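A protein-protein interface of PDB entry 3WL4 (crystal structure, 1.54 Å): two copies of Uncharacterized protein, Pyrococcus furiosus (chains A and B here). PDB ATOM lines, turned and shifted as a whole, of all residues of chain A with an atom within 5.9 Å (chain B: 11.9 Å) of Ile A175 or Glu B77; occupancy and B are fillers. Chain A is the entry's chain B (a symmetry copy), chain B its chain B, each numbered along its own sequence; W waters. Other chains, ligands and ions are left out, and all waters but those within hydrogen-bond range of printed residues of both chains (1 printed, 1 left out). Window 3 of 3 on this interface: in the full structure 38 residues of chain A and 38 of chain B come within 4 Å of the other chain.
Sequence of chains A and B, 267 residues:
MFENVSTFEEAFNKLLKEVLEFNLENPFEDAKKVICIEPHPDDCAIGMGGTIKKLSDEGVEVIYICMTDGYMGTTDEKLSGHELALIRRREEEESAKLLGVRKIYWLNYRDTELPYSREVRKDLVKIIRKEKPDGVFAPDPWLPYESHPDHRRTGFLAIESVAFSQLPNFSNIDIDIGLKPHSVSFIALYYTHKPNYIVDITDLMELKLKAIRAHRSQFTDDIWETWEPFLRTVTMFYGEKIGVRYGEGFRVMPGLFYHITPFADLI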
ATOM      1  N   ARG A 129       6.587  15.358  -4.338  1.00  0.00           N
ATOM      2  CA  ARG A 129       6.988  13.911  -4.256  1.00  0.00           C
ATOM      3  C   ARG A 129       5.772  13.137  -3.813  1.00  0.00           C
ATOM      4  O   ARG A 129       5.660  11.927  -4.259  1.00  0.00           O
ATOM      5  CB  ARG A 129       8.126  13.760  -3.246  1.00  0.00           C
ATOM      6  CG  ARG A 129       9.398  14.350  -3.813  1.00  0.00           C
ATOM      7  CD  ARG A 129      10.522  14.235  -2.712  1.00  0.00           C
ATOM      8  NE  ARG A 129      11.801  14.668  -3.318  1.00  0.00           N
ATOM      9  CZ  ARG A 129      12.909  14.973  -2.559  1.00  0.00           C
ATOM     10  NH1 ARG A 129      12.801  15.058  -1.228  1.00  0.00           N
ATOM     11  NH2 ARG A 129      14.012  15.232  -3.208  1.00  0.00           N
ATOM     12  N   LEU A 167      16.057  15.274  -6.757  1.00  0.00           N
ATOM     13  CA  LEU A 167      17.429  15.037  -6.237  1.00  0.00           C
ATOM     14  C   LEU A 167      17.334  14.394  -4.917  1.00  0.00           C
ATOM     15  O   LEU A 167      16.827  14.968  -3.903  1.00  0.00           O
ATOM     16  CB  LEU A 167      18.143  16.456  -6.001  1.00  0.00           C
ATOM     17  CG  LEU A 167      18.213  17.277  -7.243  1.00  0.00           C
ATOM     18  CD1 LEU A 167      18.928  18.643  -7.038  1.00  0.00           C
ATOM     19  CD2 LEU A 167      19.052  16.541  -8.359  1.00  0.00           C
ATOM     20  N   PRO A 168      17.816  13.137  -4.699  1.00  0.00           N
ATOM     21  CA  PRO A 168      17.585  12.435  -3.418  1.00  0.00           C
ATOM     22  C   PRO A 168      18.353  13.012  -2.187  1.00  0.00           C
ATOM     23  O   PRO A 168      17.927  12.764  -1.082  1.00  0.00           O
ATOM     24  CB  PRO A 168      18.150  11.001  -3.689  1.00  0.00           C
ATOM     25  CG  PRO A 168      18.936  11.164  -4.882  1.00  0.00           C
ATOM     26  CD  PRO A 168      18.419  12.315  -5.804  1.00  0.00           C
ATOM     27  N   ASN A 169      19.386  13.817  -2.464  1.00  0.00           N
ATOM     28  CA  ASN A 169      20.031  14.468  -1.342  1.00  0.00           C
ATOM     29  C   ASN A 169      19.397  15.792  -0.969  1.00  0.00           C
ATOM     30  O   ASN A 169      19.789  16.421   0.067  1.00  0.00           O
ATOM     31  CB  ASN A 169      21.523  14.765  -1.696  1.00  0.00           C
ATOM     32  CG  ASN A 169      22.356  13.435  -1.766  1.00  0.00           C
ATOM     33  OD1 ASN A 169      23.148  13.277  -2.686  1.00  0.00           O
ATOM     34  ND2 ASN A 169      22.096  12.600  -0.915  1.00  0.00           N
ATOM     35  N   PHE A 170      18.358  16.205  -1.749  1.00  0.00           N
ATOM     36  CA  PHE A 170      17.627  17.435  -1.355  1.00  0.00           C
ATOM     37  C   PHE A 170      16.460  16.975  -0.506  1.00  0.00           C
ATOM     38  O   PHE A 170      15.642  16.139  -0.901  1.00  0.00           O
ATOM     39  CB  PHE A 170      17.133  18.174  -2.651  1.00  0.00           C
ATOM     40  CG  PHE A 170      16.433  19.473  -2.290  1.00  0.00           C
ATOM     41  CD1 PHE A 170      17.257  20.614  -2.328  1.00  0.00           C
ATOM     42  CD2 PHE A 170      15.145  19.484  -1.898  1.00  0.00           C
ATOM     43  CE1 PHE A 170      16.652  21.893  -2.019  1.00  0.00           C
ATOM     44  CE2 PHE A 170      14.552  20.757  -1.443  1.00  0.00           C
ATOM     45  CZ  PHE A 170      15.342  21.821  -1.472  1.00  0.00           C
ATOM     46  N   SER A 171      16.319  17.578   0.696  1.00  0.00           N
ATOM     47  CA  SER A 171      15.282  17.119   1.625  1.00  0.00           C
ATOM     48  C   SER A 171      15.227  15.616   1.817  1.00  0.00           C
ATOM     49  O   SER A 171      14.221  14.964   1.562  1.00  0.00           O
ATOM     50  CB  SER A 171      13.930  17.802   1.278  1.00  0.00           C
ATOM     51  OG  SER A 171      13.103  17.833   2.426  1.00  0.00           O
ATOM     52  N   ASN A 172      16.360  15.106   2.320  1.00  0.00           N
ATOM     53  CA  ASN A 172      16.572  13.696   2.205  1.00  0.00           C
ATOM     54  C   ASN A 172      15.682  12.970   3.212  1.00  0.00           C
ATOM     55  O   ASN A 172      15.504  11.721   3.027  1.00  0.00           O
ATOM     56  CB  ASN A 172      18.095  13.338   2.481  1.00  0.00           C
ATOM     57  CG  ASN A 172      18.569  13.586   3.924  1.00  0.00           C
ATOM     58  OD1 ASN A 172      18.595  12.637   4.739  1.00  0.00           O
ATOM     59  ND2 ASN A 172      18.558  14.789   4.300  1.00  0.00           N
ATOM     60  N   ILE A 173      15.071  13.548   4.244  1.00  0.00           N
ATOM     61  CA  ILE A 173      14.250  12.778   5.153  1.00  0.00           C
ATOM     62  C   ILE A 173      12.961  12.346   4.405  1.00  0.00           C
ATOM     63  O   ILE A 173      12.372  11.332   4.748  1.00  0.00           O
ATOM     64  CB  ILE A 173      13.851  13.614   6.408  1.00  0.00           C
ATOM     65  CG1 ILE A 173      15.112  14.081   7.071  1.00  0.00           C
ATOM     66  CG2 ILE A 173      13.041  12.806   7.439  1.00  0.00           C
ATOM     67  CD1 ILE A 173      16.135  12.883   7.403  1.00  0.00           C
ATOM     68  N   ASP A 174      12.575  13.039   3.309  1.00  0.00           N
ATOM     69  CA  ASP A 174      11.401  12.584   2.536  1.00  0.00           C
ATOM     70  C   ASP A 174      11.698  11.188   2.011  1.00  0.00           C
ATOM     71  O   ASP A 174      10.805  10.361   2.099  1.00  0.00           O
ATOM     72  CB  ASP A 174      11.270  13.540   1.287  1.00  0.00           C
ATOM     73  CG  ASP A 174      10.617  14.810   1.571  1.00  0.00           C
ATOM     74  OD1 ASP A 174      10.043  14.999   2.677  1.00  0.00           O
ATOM     75  OD2 ASP A 174      10.588  15.599   0.564  1.00  0.00           O
ATOM     76  N   ILE A 175      12.891  10.955   1.497  1.00  0.00           N
ATOM     77  CA  ILE A 175      13.283   9.624   0.872  1.00  0.00           C
ATOM     78  C   ILE A 175      13.265   8.659   2.013  1.00  0.00           C
ATOM     79  O   ILE A 175      12.668   7.561   1.913  1.00  0.00           O
ATOM     80  CB  ILE A 175      14.652   9.721   0.264  1.00  0.00           C
ATOM     81  CG1 ILE A 175      14.724  10.312  -1.149  1.00  0.00           C
ATOM     82  CG2 ILE A 175      15.308   8.378   0.210  1.00  0.00           C
ATOM     83  CD1 ILE A 175      14.062  11.657  -1.392  1.00  0.00           C
ATOM     84  N   ASP A 176      13.766   9.070   3.205  1.00  0.00           N
ATOM     85  CA  ASP A 176      13.807   8.122   4.315  1.00  0.00           C
ATOM     86  C   ASP A 176      12.464   7.688   4.812  1.00  0.00           C
ATOM     87  O   ASP A 176      12.370   6.636   5.435  1.00  0.00           O
ATOM     88  CB  ASP A 176      14.584   8.741   5.518  1.00  0.00           C
ATOM     89  CG  ASP A 176      16.032   9.047   5.166  1.00  0.00           C
ATOM     90  OD1 ASP A 176      16.648   8.508   4.173  1.00  0.00           O
ATOM     91  OD2 ASP A 176      16.578   9.988   5.788  1.00  0.00           O
ATOM     92  N   ILE A 177      11.405   8.494   4.663  1.00  0.00           N
ATOM     93  CA  ILE A 177      10.054   8.123   5.104  1.00  0.00           C
ATOM     94  C   ILE A 177       9.249   7.614   3.959  1.00  0.00           C
ATOM     95  O   ILE A 177       8.061   7.381   4.146  1.00  0.00           O
ATOM     96  CB  ILE A 177       9.323   9.231   5.857  1.00  0.00           C
ATOM     97  CG1 ILE A 177       9.064  10.462   4.922  1.00  0.00           C
ATOM     98  CG2 ILE A 177      10.125   9.708   7.100  1.00  0.00           C
ATOM     99  CD1 ILE A 177       7.895  11.289   5.398  1.00  0.00           C
ATOM    100  N   GLY A 178       9.835   7.465   2.799  1.00  0.00           N
ATOM    101  CA  GLY A 178       9.200   6.759   1.627  1.00  0.00           C
ATOM    102  C   GLY A 178       8.636   7.621   0.519  1.00  0.00           C
ATOM    103  O   GLY A 178       7.905   7.158  -0.360  1.00  0.00           O
ATOM    104  N   LEU A 179       8.898   8.920   0.560  1.00  0.00           N
ATOM    105  CA  LEU A 179       8.559   9.868  -0.540  1.00  0.00           C
ATOM    106  C   LEU A 179       9.742   9.902  -1.465  1.00  0.00           C
ATOM    107  O   LEU A 179      10.732  10.689  -1.189  1.00  0.00           O
ATOM    108  CB  LEU A 179       8.279  11.316   0.013  1.00  0.00           C
ATOM    109  CG  LEU A 179       7.156  11.335   0.934  1.00  0.00           C
ATOM    110  CD1 LEU A 179       7.133  12.832   1.478  1.00  0.00           C
ATOM    111  CD2 LEU A 179       5.847  11.211   0.061  1.00  0.00           C
ATOM    112  N   LYS A 180       9.643   9.203  -2.567  1.00  0.00           N
ATOM    113  CA  LYS A 180      10.731   9.072  -3.454  1.00  0.00           C
ATOM    114  C   LYS A 180      10.937  10.351  -4.345  1.00  0.00           C
ATOM    115  O   LYS A 180       9.981  11.147  -4.512  1.00  0.00           O
ATOM    116  CB  LYS A 180      10.516   7.898  -4.425  1.00  0.00           C
ATOM    117  CG  LYS A 180      10.585   6.458  -3.707  1.00  0.00           C
ATOM    118  CD  LYS A 180      10.004   5.342  -4.741  1.00  0.00           C
ATOM    119  CE  LYS A 180       8.847   5.798  -5.817  1.00  0.00           C
ATOM    120  NZ  LYS A 180       7.381   6.039  -5.256  1.00  0.00           N
ATOM    121  N   PRO A 181      12.054  10.509  -4.994  1.00  0.00           N
ATOM    122  CA  PRO A 181      12.299  11.592  -5.938  1.00  0.00           C
ATOM    123  C   PRO A 181      11.242  11.515  -7.030  1.00  0.00           C
ATOM    124  O   PRO A 181      10.763  10.401  -7.421  1.00  0.00           O
ATOM    125  CB  PRO A 181      13.678  11.372  -6.500  1.00  0.00           C
ATOM    126  CG  PRO A 181      14.378  10.562  -5.343  1.00  0.00           C
ATOM    127  CD  PRO A 181      13.284   9.696  -4.768  1.00  0.00           C
ATOM    128  N   TYR B  71      27.321  19.291  -3.661  1.00  0.00           N
ATOM    129  CA  TYR B  71      26.666  18.217  -2.905  1.00  0.00           C
ATOM    130  C   TYR B  71      25.424  17.673  -3.524  1.00  0.00           C
ATOM    131  O   TYR B  71      25.097  16.519  -3.295  1.00  0.00           O
ATOM    132  CB  TYR B  71      26.436  18.887  -1.476  1.00  0.00           C
ATOM    133  CG  TYR B  71      25.754  18.100  -0.439  1.00  0.00           C
ATOM    134  CD1 TYR B  71      26.467  17.587   0.638  1.00  0.00           C
ATOM    135  CD2 TYR B  71      24.360  17.870  -0.461  1.00  0.00           C
ATOM    136  CE1 TYR B  71      25.832  16.906   1.737  1.00  0.00           C
ATOM    137  CE2 TYR B  71      23.710  17.220   0.522  1.00  0.00           C
ATOM    138  CZ  TYR B  71      24.457  16.749   1.622  1.00  0.00           C
ATOM    139  OH  TYR B  71      23.863  16.064   2.713  1.00  0.00           O
ATOM    140  N   MET B  72      24.657  18.513  -4.215  1.00  0.00           N
ATOM    141  CA  MET B  72      23.330  18.083  -4.652  1.00  0.00           C
ATOM    142  C   MET B  72      23.365  17.462  -6.047  1.00  0.00           C
ATOM    143  O   MET B  72      22.312  16.913  -6.465  1.00  0.00           O
ATOM    144  CB  MET B  72      22.342  19.258  -4.733  1.00  0.00           C
ATOM    145  CG  MET B  72      22.147  19.766  -3.272  1.00  0.00           C
ATOM    146  SD  MET B  72      21.051  18.565  -2.236  1.00  0.00           S
ATOM    147  CE  MET B  72      21.029  19.735  -0.661  1.00  0.00           C
ATOM    148  N   GLY B  73      24.470  17.454  -6.746  1.00  0.00           N
ATOM    149  CA  GLY B  73      24.527  17.051  -8.182  1.00  0.00           C
ATOM    150  C   GLY B  73      24.402  15.577  -8.462  1.00  0.00           C
ATOM    151  O   GLY B  73      25.354  15.027  -9.161  1.00  0.00           O
ATOM    152  N   THR B  74      23.508  14.839  -7.884  1.00  0.00           N
ATOM    153  CA  THR B  74      23.373  13.378  -8.279  1.00  0.00           C
ATOM    154  C   THR B  74      21.864  12.989  -8.213  1.00  0.00           C
ATOM    155  O   THR B  74      21.119  13.507  -7.388  1.00  0.00           O
ATOM    156  CB  THR B  74      24.194  12.461  -7.345  1.00  0.00           C
ATOM    157  OG1 THR B  74      24.019  11.021  -7.676  1.00  0.00           O
ATOM    158  CG2 THR B  74      23.724  12.503  -5.894  1.00  0.00           C
ATOM    159  N   THR B  75      21.423  12.023  -9.107  1.00  0.00           N
ATOM    160  CA  THR B  75      20.131  11.373  -8.911  1.00  0.00           C
ATOM    161  C   THR B  75      20.268   9.965  -8.374  1.00  0.00           C
ATOM    162  O   THR B  75      19.268   9.249  -8.165  1.00  0.00           O
ATOM    163  CB  THR B  75      19.308  11.402 -10.216  1.00  0.00           C
ATOM    164  OG1 THR B  75      20.086  10.754 -11.251  1.00  0.00           O
ATOM    165  CG2 THR B  75      19.099  12.818 -10.635  1.00  0.00           C
ATOM    166  N   ASP B  76      21.512   9.576  -7.980  1.00  0.00           N
ATOM    167  CA  ASP B  76      21.708   8.199  -7.365  1.00  0.00           C
ATOM    168  C   ASP B  76      21.328   8.209  -5.881  1.00  0.00           C
ATOM    169  O   ASP B  76      22.035   8.896  -5.016  1.00  0.00           O
ATOM    170  CB  ASP B  76      23.182   7.776  -7.625  1.00  0.00           C
ATOM    171  CG  ASP B  76      23.538   6.377  -6.969  1.00  0.00           C
ATOM    172  OD1 ASP B  76      22.726   5.762  -6.207  1.00  0.00           O
ATOM    173  OD2 ASP B  76      24.654   5.977  -7.152  1.00  0.00           O
ATOM    174  N   GLU B  77      20.276   7.474  -5.464  1.00  0.00           N
ATOM    175  CA  GLU B  77      19.822   7.493  -4.081  1.00  0.00           C
ATOM    176  C   GLU B  77      20.901   6.805  -3.152  1.00  0.00           C
ATOM    177  O   GLU B  77      20.848   7.003  -1.912  1.00  0.00           O
ATOM    178  CB  GLU B  77      18.507   6.773  -3.852  1.00  0.00           C
ATOM    179  CG  GLU B  77      17.183   7.463  -4.313  1.00  0.00           C
ATOM    180  CD  GLU B  77      15.903   6.630  -3.882  1.00  0.00           C
ATOM    181  OE1 GLU B  77      15.943   5.985  -2.768  1.00  0.00           O
ATOM    182  OE2 GLU B  77      14.927   6.578  -4.685  1.00  0.00           O
ATOM    183  N   LYS B  78      21.898   6.124  -3.748  1.00  0.00           N
ATOM    184  CA  LYS B  78      22.913   5.508  -2.867  1.00  0.00           C
ATOM    185  C   LYS B  78      24.128   6.430  -2.703  1.00  0.00           C
ATOM    186  O   LYS B  78      25.081   6.020  -1.951  1.00  0.00           O
ATOM    187  CB  LYS B  78      23.376   4.120  -3.415  1.00  0.00           C
ATOM    188  CG  LYS B  78      22.231   2.982  -3.244  1.00  0.00           C
ATOM    189  CD  LYS B  78      22.644   1.606  -3.983  1.00  0.00           C
ATOM    190  CE  LYS B  78      23.419   1.780  -5.398  1.00  0.00           C
ATOM    191  NZ  LYS B  78      22.733   2.696  -6.451  1.00  0.00           N
ATOM    192  N   LEU B  79      24.188   7.588  -3.367  1.00  0.00           N
ATOM    193  CA  LEU B  79      25.465   8.388  -3.280  1.00  0.00           C
ATOM    194  C   LEU B  79      25.200   9.619  -2.388  1.00  0.00           C
ATOM    195  O   LEU B  79      24.343  10.471  -2.810  1.00  0.00           O
ATOM    196  CB  LEU B  79      25.821   8.876  -4.584  1.00  0.00           C
ATOM    197  CG  LEU B  79      27.093   9.701  -4.683  1.00  0.00           C
ATOM    198  CD1 LEU B  79      28.338   8.873  -4.255  1.00  0.00           C
ATOM    199  CD2 LEU B  79      27.307  10.093  -6.135  1.00  0.00           C
ATOM    200  N   SER B  80      25.871   9.651  -1.262  1.00  0.00           N
ATOM    201  CA  SER B  80      25.532  10.782  -0.323  1.00  0.00           C
ATOM    202  C   SER B  80      26.123  12.027  -0.964  1.00  0.00           C
ATOM    203  O   SER B  80      27.088  12.063  -1.749  1.00  0.00           O
ATOM    204  CB  SER B  80      26.145  10.517   1.044  1.00  0.00           C
ATOM    205  OG  SER B  80      27.582  10.619   1.001  1.00  0.00           O
ATOM    206  N   GLY B  81      25.611  13.184  -0.443  1.00  0.00           N
ATOM    207  CA  GLY B  81      26.203  14.444  -0.917  1.00  0.00           C
ATOM    208  C   GLY B  81      27.660  14.681  -0.496  1.00  0.00           C
ATOM    209  O   GLY B  81      28.452  15.351  -1.139  1.00  0.00           O
ATOM    210  N   HIS B  82      27.992  14.119   0.704  1.00  0.00           N
ATOM    211  CA  HIS B  82      29.376  14.207   1.175  1.00  0.00           C
ATOM    212  C   HIS B  82      30.376  13.450   0.249  1.00  0.00           C
ATOM    213  O   HIS B  82      31.400  14.016  -0.122  1.00  0.00           O
ATOM    214  CB  HIS B  82      29.463  13.598   2.573  1.00  0.00           C
ATOM    215  CG  HIS B  82      28.495  14.160   3.568  1.00  0.00           C
ATOM    216  ND1 HIS B  82      28.519  15.510   3.922  1.00  0.00           N
ATOM    217  CD2 HIS B  82      27.526  13.573   4.287  1.00  0.00           C
ATOM    218  CE1 HIS B  82      27.548  15.693   4.792  1.00  0.00           C
ATOM    219  NE2 HIS B  82      26.921  14.565   5.046  1.00  0.00           N
ATOM    220  N   GLU B  83      29.913  12.266  -0.125  1.00  0.00           N
ATOM    221  CA  GLU B  83      30.789  11.514  -1.030  1.00  0.00           C
ATOM    222  C   GLU B  83      30.870  12.174  -2.401  1.00  0.00           C
ATOM    223  O   GLU B  83      31.923  12.293  -2.968  1.00  0.00           O
ATOM    224  CB  GLU B  83      30.263  10.032  -1.184  1.00  0.00           C
ATOM    225  CG  GLU B  83      31.355   9.255  -2.003  1.00  0.00           C
ATOM    226  CD  GLU B  83      31.068   7.733  -1.942  1.00  0.00           C
ATOM    227  OE1 GLU B  83      30.105   7.262  -1.338  1.00  0.00           O
ATOM    228  OE2 GLU B  83      31.904   7.086  -2.646  1.00  0.00           O
ATOM    229  N   LEU B  84      29.725  12.709  -2.899  1.00  0.00           N
ATOM    230  CA  LEU B  84      29.739  13.411  -4.167  1.00  0.00           C
ATOM    231  C   LEU B  84      30.660  14.618  -4.117  1.00  0.00           C
ATOM    232  O   LEU B  84      31.424  14.900  -4.994  1.00  0.00           O
ATOM    233  CB  LEU B  84      28.314  13.829  -4.561  1.00  0.00           C
ATOM    234  CG  LEU B  84      28.330  14.624  -5.800  1.00  0.00           C
ATOM    235  CD1 LEU B  84      28.755  13.803  -7.073  1.00  0.00           C
ATOM    236  CD2 LEU B  84      26.815  15.011  -6.108  1.00  0.00           C
ATOM    237  N   SER B 217      31.073  12.618 -12.747  1.00  0.00           N
ATOM    238  CA  SER B 217      29.900  12.418 -11.951  1.00  0.00           C
ATOM    239  C   SER B 217      28.675  13.239 -12.538  1.00  0.00           C
ATOM    240  O   SER B 217      27.503  12.851 -12.270  1.00  0.00           O
ATOM    241  CB  SER B 217      30.138  12.896 -10.470  1.00  0.00           C
ATOM    242  OG  SER B 217      30.352  14.300 -10.482  1.00  0.00           O
HETATM  243  O   HOH W   1      20.937  14.711  -4.941  1.00  0.00           O
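No position is printed for both chains.
Of the printed residues of chain B, Leu A167 touches Met B72 and Thr B74. Printed residues of chain B within 4 Å of Asn A169: Tyr B71, Met B72, Thr B74, Leu B79, Ser B80 and Gly B81. Of the printed residues of chain B, Phe A170 touches Met B72 (3.6 Å). No residue of chain B comes within 4 Å of Asn A172. Ile A173 touches none of the printed residues of chain B. No residue of chain B comes within 4 Å of Asp A174. Printed residues of chain B within 4 Å of Ile A175: Glu B77. No residue of chain B comes within 4 Å of Asp A176. No residue of chain B comes within 4 Å of Ile A177. No residue of chain B comes within 4 Å of Gly A178. No residue of chain B comes within 4 Å of Leu A179. Lys A180 touches none of the printed residues of chain B. Of chain B, only Glu B77 (3.5 Å) comes within 4 Å of Pro A181. Of the printed residues of chain A, Tyr B71 touches Asn A169. Printed residues of chain A within 4 Å of Asp B76: Pro A168 (3.8 Å). Of chain A, only Pro A168 (3.7 Å), Ile A175 (3.9 Å) and Pro A181 (3.5 Å) come within 4 Å of Glu B77. The nearest residue of chain B that does not touch Ile A175 is Lys B78 (8.0 Å). The nearest residue of chain A that does not touch Glu B77 is Lys A180 (4.5 Å). The nearest printed residue of chain A that does not touch Asp B76 is Asn A169 (5.1 Å).
OD1 of Asp B76 is in salt-bridge range of NZ of Lys B78, 3.1 Å away. The side-chain hydroxyl of Ser B80 sits at hydrogen-bond distance from the backbone NH of Glu B83 (3.1 Å). The backbone NH of Asp B76 sits at hydrogen-bond distance from the side-chain hydroxyl of Thr B74 (2.9 Å). NH2 of Arg A129 is in hydrogen-bond range of O of Phe A170, at 3.0 Å. The backbone carbonyl oxygen (O) of Leu A167 sits at hydrogen-bond distance from the guanidinium group (NH2) of Arg A129 (2.9 Å).
Of the 15 printed residues of chain B, 9 touch a printed residue of chain A. Along chain B the printed residues that touch a printed residue of chain A span positions 71 to 81. Among the printed residues, no Asp or Glu carboxylate lies within 4 Å of a Lys or Arg side-chain nitrogen of the other chain.
Water W1 lies within hydrogen-bond range of O of Thr B74 (2.7 Å), O of Met B72 (3.0 Å) and N of Asn A169 (3.1 Å).
The side-chain amide oxygen of Asn A169 lies close to the backbone carbonyl oxygen of Leu B79, 3.1 Å away. The backbone carbonyl oxygen of Asn A169 sits close to the side-chain sulfur of Met B72. N of Gly B81 sits at hydrogen-bond distance from OD1 of Asn A169 (3.3 Å). SD of Met B72 sits at hydrogen-bond distance from N of Phe A170, at 3.6 Å.
Among the printed residues, pairs that only touch across the chains: Pro A168 with Thr B74, Asn A169 with Thr B74, Pro A181 with Glu B77, Asn A169 with Ser B80, Pro A168 with Thr B75, Pro A168 with Glu B77, Leu A167 with Met B72, Leu A167 with Thr B74, Asn A169 with Tyr B71, Pro A168 with Asp B76 and Ile A175 with Glu B77.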
